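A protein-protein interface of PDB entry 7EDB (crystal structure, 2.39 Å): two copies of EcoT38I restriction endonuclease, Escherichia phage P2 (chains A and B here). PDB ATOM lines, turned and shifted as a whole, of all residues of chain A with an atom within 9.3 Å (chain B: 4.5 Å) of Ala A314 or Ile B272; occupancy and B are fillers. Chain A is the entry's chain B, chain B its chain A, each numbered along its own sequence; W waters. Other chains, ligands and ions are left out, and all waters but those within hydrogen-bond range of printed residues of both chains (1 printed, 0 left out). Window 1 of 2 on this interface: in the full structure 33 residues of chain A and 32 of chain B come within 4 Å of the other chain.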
ATOM      1  N   PHE A 178     -26.022 -11.364  16.884  1.00  0.00           N
ATOM      2  CA  PHE A 178     -24.756 -12.078  16.759  1.00  0.00           C
ATOM      3  C   PHE A 178     -24.256 -12.072  15.322  1.00  0.00           C
ATOM      4  O   PHE A 178     -23.063 -11.861  15.081  1.00  0.00           O
ATOM      5  CB  PHE A 178     -24.898 -13.509  17.263  1.00  0.00           C
ATOM      6  CG  PHE A 178     -23.600 -14.265  17.296  1.00  0.00           C
ATOM      7  CD1 PHE A 178     -22.571 -13.860  18.138  1.00  0.00           C
ATOM      8  CD2 PHE A 178     -23.403 -15.375  16.488  1.00  0.00           C
ATOM      9  CE1 PHE A 178     -21.367 -14.554  18.179  1.00  0.00           C
ATOM     10  CE2 PHE A 178     -22.208 -16.088  16.530  1.00  0.00           C
ATOM     11  CZ  PHE A 178     -21.187 -15.679  17.378  1.00  0.00           C
ATOM     12  N   HIS A 179     -25.151 -12.290  14.353  1.00  0.00           N
ATOM     13  CA  HIS A 179     -24.731 -12.317  12.955  1.00  0.00           C
ATOM     14  C   HIS A 179     -23.997 -11.044  12.570  1.00  0.00           C
ATOM     15  O   HIS A 179     -23.013 -11.087  11.822  1.00  0.00           O
ATOM     16  CB  HIS A 179     -25.932 -12.516  12.032  1.00  0.00           C
ATOM     17  CG  HIS A 179     -25.594 -12.354  10.582  1.00  0.00           C
ATOM     18  ND1 HIS A 179     -24.999 -13.351   9.838  1.00  0.00           N
ATOM     19  CD2 HIS A 179     -25.738 -11.298   9.748  1.00  0.00           C
ATOM     20  CE1 HIS A 179     -24.807 -12.923   8.602  1.00  0.00           C
ATOM     21  NE2 HIS A 179     -25.246 -11.681   8.521  1.00  0.00           N
ATOM     22  N   SER A 202     -17.532 -18.037  19.525  1.00  0.00           N
ATOM     23  CA  SER A 202     -18.728 -18.856  19.381  1.00  0.00           C
ATOM     24  C   SER A 202     -18.619 -20.110  20.223  1.00  0.00           C
ATOM     25  O   SER A 202     -19.600 -20.541  20.838  1.00  0.00           O
ATOM     26  CB  SER A 202     -18.943 -19.216  17.923  1.00  0.00           C
ATOM     27  OG  SER A 202     -18.832 -18.043  17.154  1.00  0.00           O
ATOM     28  N   LEU A 205     -19.377 -19.074  23.763  1.00  0.00           N
ATOM     29  CA  LEU A 205     -20.810 -18.906  24.007  1.00  0.00           C
ATOM     30  C   LEU A 205     -21.482 -20.244  24.260  1.00  0.00           C
ATOM     31  O   LEU A 205     -22.347 -20.360  25.134  1.00  0.00           O
ATOM     32  CB  LEU A 205     -21.483 -18.195  22.828  1.00  0.00           C
ATOM     33  CG  LEU A 205     -21.068 -16.736  22.612  1.00  0.00           C
ATOM     34  CD1 LEU A 205     -21.409 -16.285  21.212  1.00  0.00           C
ATOM     35  CD2 LEU A 205     -21.712 -15.819  23.623  1.00  0.00           C
ATOM     36  N   LEU A 206     -21.071 -21.274  23.522  1.00  0.00           N
ATOM     37  CA  LEU A 206     -21.749 -22.559  23.588  1.00  0.00           C
ATOM     38  C   LEU A 206     -21.270 -23.389  24.769  1.00  0.00           C
ATOM     39  O   LEU A 206     -22.061 -24.125  25.368  1.00  0.00           O
ATOM     40  CB  LEU A 206     -21.546 -23.314  22.275  1.00  0.00           C
ATOM     41  CG  LEU A 206     -22.228 -24.671  22.144  1.00  0.00           C
ATOM     42  CD1 LEU A 206     -23.712 -24.525  22.448  1.00  0.00           C
ATOM     43  CD2 LEU A 206     -22.004 -25.209  20.749  1.00  0.00           C
ATOM     44  N   ARG A 210     -21.232 -25.685  29.720  1.00  0.00           N
ATOM     45  CA  ARG A 210     -20.987 -27.101  29.491  1.00  0.00           C
ATOM     46  C   ARG A 210     -19.645 -27.553  30.037  1.00  0.00           C
ATOM     47  O   ARG A 210     -19.274 -28.713  29.840  1.00  0.00           O
ATOM     48  CB  ARG A 210     -21.070 -27.424  27.992  1.00  0.00           C
ATOM     49  CG  ARG A 210     -22.412 -27.065  27.361  1.00  0.00           C
ATOM     50  CD  ARG A 210     -22.439 -27.347  25.859  1.00  0.00           C
ATOM     51  NE  ARG A 210     -23.745 -27.026  25.271  1.00  0.00           N
ATOM     52  CZ  ARG A 210     -24.646 -27.931  24.892  1.00  0.00           C
ATOM     53  NH1 ARG A 210     -24.401 -29.226  25.026  1.00  0.00           N
ATOM     54  NH2 ARG A 210     -25.798 -27.543  24.374  1.00  0.00           N
ATOM     55  N   MET A 306     -18.850 -18.539   8.955  1.00  0.00           N
ATOM     56  CA  MET A 306     -20.121 -17.923   9.314  1.00  0.00           C
ATOM     57  C   MET A 306     -21.163 -18.972   9.700  1.00  0.00           C
ATOM     58  O   MET A 306     -21.910 -18.788  10.673  1.00  0.00           O
ATOM     59  CB  MET A 306     -20.621 -17.060   8.159  1.00  0.00           C
ATOM     60  CG  MET A 306     -22.005 -16.446   8.401  1.00  0.00           C
ATOM     61  SD  MET A 306     -22.002 -15.173   9.683  1.00  0.00           S
ATOM     62  CE  MET A 306     -20.952 -13.933   8.926  1.00  0.00           C
ATOM     63  N   THR A 307     -21.241 -20.068   8.943  1.00  0.00           N
ATOM     64  CA  THR A 307     -22.191 -21.124   9.277  1.00  0.00           C
ATOM     65  C   THR A 307     -21.890 -21.709  10.647  1.00  0.00           C
ATOM     66  O   THR A 307     -22.806 -21.955  11.441  1.00  0.00           O
ATOM     67  CB  THR A 307     -22.156 -22.230   8.219  1.00  0.00           C
ATOM     68  OG1 THR A 307     -22.403 -21.676   6.923  1.00  0.00           O
ATOM     69  CG2 THR A 307     -23.195 -23.291   8.527  1.00  0.00           C
ATOM     70  N   PHE A 308     -20.605 -21.924  10.942  1.00  0.00           N
ATOM     71  CA  PHE A 308     -20.202 -22.534  12.203  1.00  0.00           C
ATOM     72  C   PHE A 308     -20.476 -21.613  13.377  1.00  0.00           C
ATOM     73  O   PHE A 308     -21.048 -22.037  14.385  1.00  0.00           O
ATOM     74  CB  PHE A 308     -18.715 -22.902  12.169  1.00  0.00           C
ATOM     75  CG  PHE A 308     -18.197 -23.430  13.480  1.00  0.00           C
ATOM     76  CD1 PHE A 308     -18.374 -24.770  13.825  1.00  0.00           C
ATOM     77  CD2 PHE A 308     -17.540 -22.589  14.375  1.00  0.00           C
ATOM     78  CE1 PHE A 308     -17.893 -25.271  15.039  1.00  0.00           C
ATOM     79  CE2 PHE A 308     -17.059 -23.078  15.592  1.00  0.00           C
ATOM     80  CZ  PHE A 308     -17.238 -24.428  15.923  1.00  0.00           C
ATOM     81  N   THR A 309     -20.061 -20.349  13.273  1.00  0.00           N
ATOM     82  CA  THR A 309     -20.262 -19.437  14.390  1.00  0.00           C
ATOM     83  C   THR A 309     -21.745 -19.248  14.690  1.00  0.00           C
ATOM     84  O   THR A 309     -22.148 -19.254  15.863  1.00  0.00           O
ATOM     85  CB  THR A 309     -19.580 -18.091  14.115  1.00  0.00           C
ATOM     86  OG1 THR A 309     -20.126 -17.488  12.935  1.00  0.00           O
ATOM     87  CG2 THR A 309     -18.066 -18.280  13.958  1.00  0.00           C
ATOM     88  N   THR A 310     -22.582 -19.100  13.651  1.00  0.00           N
ATOM     89  CA  THR A 310     -24.004 -18.851  13.916  1.00  0.00           C
ATOM     90  C   THR A 310     -24.745 -20.117  14.317  1.00  0.00           C
ATOM     91  O   THR A 310     -25.764 -20.030  15.010  1.00  0.00           O
ATOM     92  CB  THR A 310     -24.700 -18.213  12.708  1.00  0.00           C
ATOM     93  OG1 THR A 310     -24.592 -19.068  11.559  1.00  0.00           O
ATOM     94  CG2 THR A 310     -24.098 -16.854  12.404  1.00  0.00           C
ATOM     95  N   THR A 311     -24.248 -21.293  13.920  1.00  0.00           N
ATOM     96  CA  THR A 311     -24.822 -22.526  14.448  1.00  0.00           C
ATOM     97  C   THR A 311     -24.525 -22.668  15.935  1.00  0.00           C
ATOM     98  O   THR A 311     -25.415 -23.030  16.713  1.00  0.00           O
ATOM     99  CB  THR A 311     -24.315 -23.727  13.655  1.00  0.00           C
ATOM    100  OG1 THR A 311     -24.894 -23.682  12.349  1.00  0.00           O
ATOM    101  CG2 THR A 311     -24.702 -25.048  14.325  1.00  0.00           C
ATOM    102  N   CYS A 312     -23.292 -22.352  16.355  1.00  0.00           N
ATOM    103  CA  CYS A 312     -22.976 -22.376  17.781  1.00  0.00           C
ATOM    104  C   CYS A 312     -23.853 -21.394  18.545  1.00  0.00           C
ATOM    105  O   CYS A 312     -24.372 -21.719  19.616  1.00  0.00           O
ATOM    106  CB  CYS A 312     -21.492 -22.060  18.028  1.00  0.00           C
ATOM    107  SG  CYS A 312     -20.292 -23.290  17.429  1.00  0.00           S
ATOM    108  N   TYR A 313     -24.038 -20.183  18.010  1.00  0.00           N
ATOM    109  CA  TYR A 313     -24.872 -19.219  18.714  1.00  0.00           C
ATOM    110  C   TYR A 313     -26.312 -19.703  18.805  1.00  0.00           C
ATOM    111  O   TYR A 313     -26.936 -19.611  19.866  1.00  0.00           O
ATOM    112  CB  TYR A 313     -24.813 -17.855  18.036  1.00  0.00           C
ATOM    113  CG  TYR A 313     -25.685 -16.859  18.742  1.00  0.00           C
ATOM    114  CD1 TYR A 313     -25.291 -16.301  19.953  1.00  0.00           C
ATOM    115  CD2 TYR A 313     -26.929 -16.508  18.227  1.00  0.00           C
ATOM    116  CE1 TYR A 313     -26.110 -15.405  20.627  1.00  0.00           C
ATOM    117  CE2 TYR A 313     -27.749 -15.609  18.885  1.00  0.00           C
ATOM    118  CZ  TYR A 313     -27.339 -15.061  20.083  1.00  0.00           C
ATOM    119  OH  TYR A 313     -28.168 -14.172  20.740  1.00  0.00           O
ATOM    120  N   ALA A 314     -26.855 -20.233  17.707  1.00  0.00           N
ATOM    121  CA  ALA A 314     -28.232 -20.715  17.734  1.00  0.00           C
ATOM    122  C   ALA A 314     -28.435 -21.787  18.797  1.00  0.00           C
ATOM    123  O   ALA A 314     -29.518 -21.892  19.375  1.00  0.00           O
ATOM    124  CB  ALA A 314     -28.628 -21.247  16.357  1.00  0.00           C
ATOM    125  N   LEU A 315     -27.406 -22.579  19.076  1.00  0.00           N
ATOM    126  CA  LEU A 315     -27.493 -23.625  20.082  1.00  0.00           C
ATOM    127  C   LEU A 315     -27.195 -23.120  21.487  1.00  0.00           C
ATOM    128  O   LEU A 315     -27.349 -23.881  22.445  1.00  0.00           O
ATOM    129  CB  LEU A 315     -26.526 -24.758  19.722  1.00  0.00           C
ATOM    130  CG  LEU A 315     -26.891 -25.457  18.408  1.00  0.00           C
ATOM    131  CD1 LEU A 315     -25.749 -26.311  17.896  1.00  0.00           C
ATOM    132  CD2 LEU A 315     -28.131 -26.303  18.616  1.00  0.00           C
ATOM    133  N   SER A 316     -26.772 -21.861  21.621  1.00  0.00           N
ATOM    134  CA  SER A 316     -26.261 -21.290  22.858  1.00  0.00           C
ATOM    135  C   SER A 316     -27.371 -20.801  23.777  1.00  0.00           C
ATOM    136  O   SER A 316     -28.510 -20.588  23.347  1.00  0.00           O
ATOM    137  CB  SER A 316     -25.337 -20.117  22.546  1.00  0.00           C
ATOM    138  OG  SER A 316     -24.042 -20.574  22.191  1.00  0.00           O
ATOM    139  N   PRO A 317     -27.061 -20.626  25.058  1.00  0.00           N
ATOM    140  CA  PRO A 317     -27.955 -19.868  25.941  1.00  0.00           C
ATOM    141  C   PRO A 317     -27.773 -18.366  25.765  1.00  0.00           C
ATOM    142  O   PRO A 317     -26.676 -17.871  25.475  1.00  0.00           O
ATOM    143  CB  PRO A 317     -27.526 -20.314  27.343  1.00  0.00           C
ATOM    144  CG  PRO A 317     -26.064 -20.706  27.172  1.00  0.00           C
ATOM    145  CD  PRO A 317     -25.955 -21.276  25.789  1.00  0.00           C
ATOM    146  N   LEU A 318     -28.880 -17.636  25.947  1.00  0.00           N
ATOM    147  CA  LEU A 318     -28.831 -16.180  25.838  1.00  0.00           C
ATOM    148  C   LEU A 318     -27.921 -15.547  26.895  1.00  0.00           C
ATOM    149  O   LEU A 318     -27.366 -14.463  26.662  1.00  0.00           O
ATOM    150  CB  LEU A 318     -30.240 -15.595  25.940  1.00  0.00           C
ATOM    151  CG  LEU A 318     -30.947 -15.274  24.624  1.00  0.00           C
ATOM    152  CD1 LEU A 318     -32.110 -14.343  24.876  1.00  0.00           C
ATOM    153  CD2 LEU A 318     -29.972 -14.675  23.622  1.00  0.00           C
ATOM    154  N   ASN A 321     -24.204 -13.866  26.465  1.00  0.00           N
ATOM    155  CA  ASN A 321     -23.944 -12.647  25.713  1.00  0.00           C
ATOM    156  C   ASN A 321     -23.314 -11.543  26.557  1.00  0.00           C
ATOM    157  O   ASN A 321     -22.685 -10.645  25.990  1.00  0.00           O
ATOM    158  CB  ASN A 321     -25.245 -12.161  25.065  1.00  0.00           C
ATOM    159  CG  ASN A 321     -25.791 -13.154  24.042  1.00  0.00           C
ATOM    160  OD1 ASN A 321     -25.055 -14.001  23.527  1.00  0.00           O
ATOM    161  ND2 ASN A 321     -27.083 -13.047  23.735  1.00  0.00           N
ATOM    162  N   LEU B 242     -35.394 -22.320  20.872  1.00  0.00           N
ATOM    163  CA  LEU B 242     -34.895 -22.472  19.514  1.00  0.00           C
ATOM    164  C   LEU B 242     -35.919 -23.259  18.706  1.00  0.00           C
ATOM    165  O   LEU B 242     -36.410 -24.289  19.175  1.00  0.00           O
ATOM    166  CB  LEU B 242     -33.549 -23.211  19.521  1.00  0.00           C
ATOM    167  CG  LEU B 242     -32.508 -23.257  18.394  1.00  0.00           C
ATOM    168  CD1 LEU B 242     -31.858 -24.668  18.312  1.00  0.00           C
ATOM    169  CD2 LEU B 242     -32.981 -22.782  17.042  1.00  0.00           C
ATOM    170  N   SER B 243     -36.220 -22.797  17.495  1.00  0.00           N
ATOM    171  CA  SER B 243     -37.017 -23.561  16.548  1.00  0.00           C
ATOM    172  C   SER B 243     -36.253 -23.742  15.249  1.00  0.00           C
ATOM    173  O   SER B 243     -35.456 -22.883  14.862  1.00  0.00           O
ATOM    174  CB  SER B 243     -38.361 -22.888  16.249  1.00  0.00           C
ATOM    175  OG  SER B 243     -39.175 -22.934  17.390  1.00  0.00           O
ATOM    176  N   ILE B 244     -36.520 -24.859  14.571  1.00  0.00           N
ATOM    177  CA  ILE B 244     -35.832 -25.225  13.341  1.00  0.00           C
ATOM    178  C   ILE B 244     -36.867 -25.380  12.235  1.00  0.00           C
ATOM    179  O   ILE B 244     -37.884 -26.057  12.419  1.00  0.00           O
ATOM    180  CB  ILE B 244     -35.011 -26.526  13.512  1.00  0.00           C
ATOM    181  CG1 ILE B 244     -33.817 -26.306  14.437  1.00  0.00           C
ATOM    182  CG2 ILE B 244     -34.494 -27.028  12.178  1.00  0.00           C
ATOM    183  CD1 ILE B 244     -34.079 -26.700  15.824  1.00  0.00           C
ATOM    184  N   GLU B 245     -36.603 -24.760  11.093  1.00  0.00           N
ATOM    185  CA  GLU B 245     -37.325 -25.025   9.856  1.00  0.00           C
ATOM    186  C   GLU B 245     -36.407 -25.805   8.924  1.00  0.00           C
ATOM    187  O   GLU B 245     -35.304 -25.346   8.617  1.00  0.00           O
ATOM    188  CB  GLU B 245     -37.767 -23.723   9.186  1.00  0.00           C
ATOM    189  CG  GLU B 245     -38.373 -23.910   7.801  1.00  0.00           C
ATOM    190  CD  GLU B 245     -39.736 -24.616   7.815  1.00  0.00           C
ATOM    191  OE1 GLU B 245     -40.025 -25.373   6.853  1.00  0.00           O
ATOM    192  OE2 GLU B 245     -40.523 -24.407   8.773  1.00  0.00           O
ATOM    193  N   LYS B 270     -34.704 -17.486  18.547  1.00  0.00           N
ATOM    194  CA  LYS B 270     -33.677 -18.108  17.714  1.00  0.00           C
ATOM    195  C   LYS B 270     -34.297 -19.110  16.748  1.00  0.00           C
ATOM    196  O   LYS B 270     -35.081 -19.978  17.147  1.00  0.00           O
ATOM    197  CB  LYS B 270     -32.595 -18.763  18.569  1.00  0.00           C
ATOM    198  CG  LYS B 270     -31.804 -17.758  19.419  1.00  0.00           C
ATOM    199  CD  LYS B 270     -30.645 -18.435  20.158  1.00  0.00           C
ATOM    200  CE  LYS B 270     -29.824 -17.406  20.952  1.00  0.00           C
ATOM    201  NZ  LYS B 270     -28.587 -17.950  21.621  1.00  0.00           N
ATOM    202  N   VAL B 271     -33.953 -18.972  15.472  1.00  0.00           N
ATOM    203  CA  VAL B 271     -34.411 -19.876  14.431  1.00  0.00           C
ATOM    204  C   VAL B 271     -33.210 -20.329  13.609  1.00  0.00           C
ATOM    205  O   VAL B 271     -32.382 -19.502  13.204  1.00  0.00           O
ATOM    206  CB  VAL B 271     -35.455 -19.207  13.522  1.00  0.00           C
ATOM    207  CG1 VAL B 271     -35.699 -20.073  12.289  1.00  0.00           C
ATOM    208  CG2 VAL B 271     -36.742 -18.986  14.285  1.00  0.00           C
ATOM    209  N   ILE B 272     -33.112 -21.639  13.375  1.00  0.00           N
ATOM    210  CA  ILE B 272     -32.201 -22.202  12.386  1.00  0.00           C
ATOM    211  C   ILE B 272     -33.016 -22.673  11.196  1.00  0.00           C
ATOM    212  O   ILE B 272     -33.981 -23.433  11.352  1.00  0.00           O
ATOM    213  CB  ILE B 272     -31.377 -23.379  12.923  1.00  0.00           C
ATOM    214  CG1 ILE B 272     -30.710 -23.047  14.236  1.00  0.00           C
ATOM    215  CG2 ILE B 272     -30.311 -23.775  11.901  1.00  0.00           C
ATOM    216  CD1 ILE B 272     -29.671 -24.136  14.624  1.00  0.00           C
ATOM    217  N   PHE B 273     -32.594 -22.263  10.016  1.00  0.00           N
ATOM    218  CA  PHE B 273     -33.206 -22.640   8.756  1.00  0.00           C
ATOM    219  C   PHE B 273     -32.230 -23.591   8.049  1.00  0.00           C
ATOM    220  O   PHE B 273     -31.145 -23.174   7.624  1.00  0.00           O
ATOM    221  CB  PHE B 273     -33.475 -21.378   7.953  1.00  0.00           C
ATOM    222  CG  PHE B 273     -34.452 -21.547   6.844  1.00  0.00           C
ATOM    223  CD1 PHE B 273     -34.071 -22.150   5.644  1.00  0.00           C
ATOM    224  CD2 PHE B 273     -35.746 -21.055   6.971  1.00  0.00           C
ATOM    225  CE1 PHE B 273     -34.976 -22.271   4.595  1.00  0.00           C
ATOM    226  CE2 PHE B 273     -36.651 -21.181   5.940  1.00  0.00           C
ATOM    227  CZ  PHE B 273     -36.267 -21.789   4.751  1.00  0.00           C
ATOM    228  N   LEU B 274     -32.606 -24.867   7.950  1.00  0.00           N
ATOM    229  CA  LEU B 274     -31.747 -25.911   7.398  1.00  0.00           C
ATOM    230  C   LEU B 274     -32.141 -26.231   5.961  1.00  0.00           C
ATOM    231  O   LEU B 274     -33.321 -26.446   5.663  1.00  0.00           O
ATOM    232  CB  LEU B 274     -31.820 -27.177   8.256  1.00  0.00           C
ATOM    233  CG  LEU B 274     -31.282 -26.979   9.676  1.00  0.00           C
ATOM    234  CD1 LEU B 274     -31.448 -28.224  10.498  1.00  0.00           C
ATOM    235  CD2 LEU B 274     -29.834 -26.572   9.640  1.00  0.00           C
ATOM    236  N   SER B 301     -30.428 -17.984  11.479  1.00  0.00           N
ATOM    237  CA  SER B 301     -29.203 -18.474  10.858  1.00  0.00           C
ATOM    238  C   SER B 301     -29.532 -19.577   9.864  1.00  0.00           C
ATOM    239  O   SER B 301     -30.601 -20.189   9.916  1.00  0.00           O
ATOM    240  CB  SER B 301     -28.194 -18.977  11.898  1.00  0.00           C
ATOM    241  OG  SER B 301     -28.680 -20.124  12.555  1.00  0.00           O
ATOM    242  N   PHE B 308     -24.821 -29.092   9.438  1.00  0.00           N
ATOM    243  CA  PHE B 308     -25.379 -29.015  10.784  1.00  0.00           C
ATOM    244  C   PHE B 308     -25.162 -30.321  11.546  1.00  0.00           C
ATOM    245  O   PHE B 308     -24.783 -30.298  12.721  1.00  0.00           O
ATOM    246  CB  PHE B 308     -26.870 -28.657  10.718  1.00  0.00           C
ATOM    247  CG  PHE B 308     -27.543 -28.543  12.071  1.00  0.00           C
ATOM    248  CD1 PHE B 308     -27.362 -27.413  12.861  1.00  0.00           C
ATOM    249  CD2 PHE B 308     -28.383 -29.552  12.534  1.00  0.00           C
ATOM    250  CE1 PHE B 308     -27.973 -27.307  14.099  1.00  0.00           C
ATOM    251  CE2 PHE B 308     -29.011 -29.453  13.771  1.00  0.00           C
ATOM    252  CZ  PHE B 308     -28.804 -28.329  14.555  1.00  0.00           C
HETATM  253  O   HOH W   1     -26.129 -21.476  11.089  1.00  0.00           O
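Thr A310 touches Ser B301 (OG1 to CB, 3.6 Å). Phe B308 touches Thr A311. Ala A314 touches Leu B242. Ala A314 touches Lys B270. Ala A314 touches Ile B272. CB of Ala A314 touches OG of Ser B301, at 3.96 Å. Lys B270 touches Leu A318.
Water W1 lies within hydrogen-bond range of the side-chain hydroxyl (OG1) of Thr A311, the side-chain hydroxyl (OG1) of Thr A310, the side-chain hydroxyl (OG) of Ser B301 and the backbone carbonyl oxygen (O) of Thr A307.
O of Tyr A313 sits at hydrogen-bond distance from NZ of Lys B270, at 2.9 Å. NZ of Lys B270 lies within hydrogen-bond range of O of Ser A316, 3.2 Å away.
The backbone carbonyl oxygen (O) of Thr A307 lies within hydrogen-bond range of the side-chain hydroxyl (OG1) of Thr A310, at 3.4 Å. OG1 of Thr A311 lies within hydrogen-bond range of O of Thr A307, 2.9 Å away. The side-chain hydroxyl (OG1) of Thr A310 lies within hydrogen-bond range of the backbone carbonyl oxygen (O) of Met A306. OG of Ser A316 lies within hydrogen-bond range of N of Leu A206 (3.3 Å). The backbone NH (N) of Ser B243 lies within hydrogen-bond range of the backbone carbonyl oxygen (O) of Lys B270 (3.1 Å). The backbone carbonyl oxygen (O) of Ile B272 lies within hydrogen-bond range of the backbone NH (N) of Glu B245.
1 position is printed for both chains. Of the 9 pairs that touch across the chains among the printed residues, none has its exchanged pair printed and touching as well.
Among the printed residues, no Asp or Glu carboxylate lies within 4 Å of a Lys or Arg side-chain nitrogen of the other chain.
Of chain B, only Leu B242, Lys B270, Ile B272 and Ser B301 come within 4 Å of Ala A314. No residue of chain A comes within 4 Å of Val B271. Of chain A, only Thr A310 (3.6 Å) and Ala A314 (3.96 Å) come within 4 Å of Ser B301. Of the printed residues of chain B, Leu A318 touches Lys B270 (3.8 Å). Printed residues of chain B within 4 Å of Ser A316: Lys B270 (3.2 Å). Printed residues of chain A within 4 Å of Phe B308: Thr A311 (3.8 Å). The nearest residue of chain A that does not touch Ile B272 is Leu A315 (4.8 Å). The nearest printed residue of chain B that does not touch Ser A316 is Leu B242 (6.7 Å).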
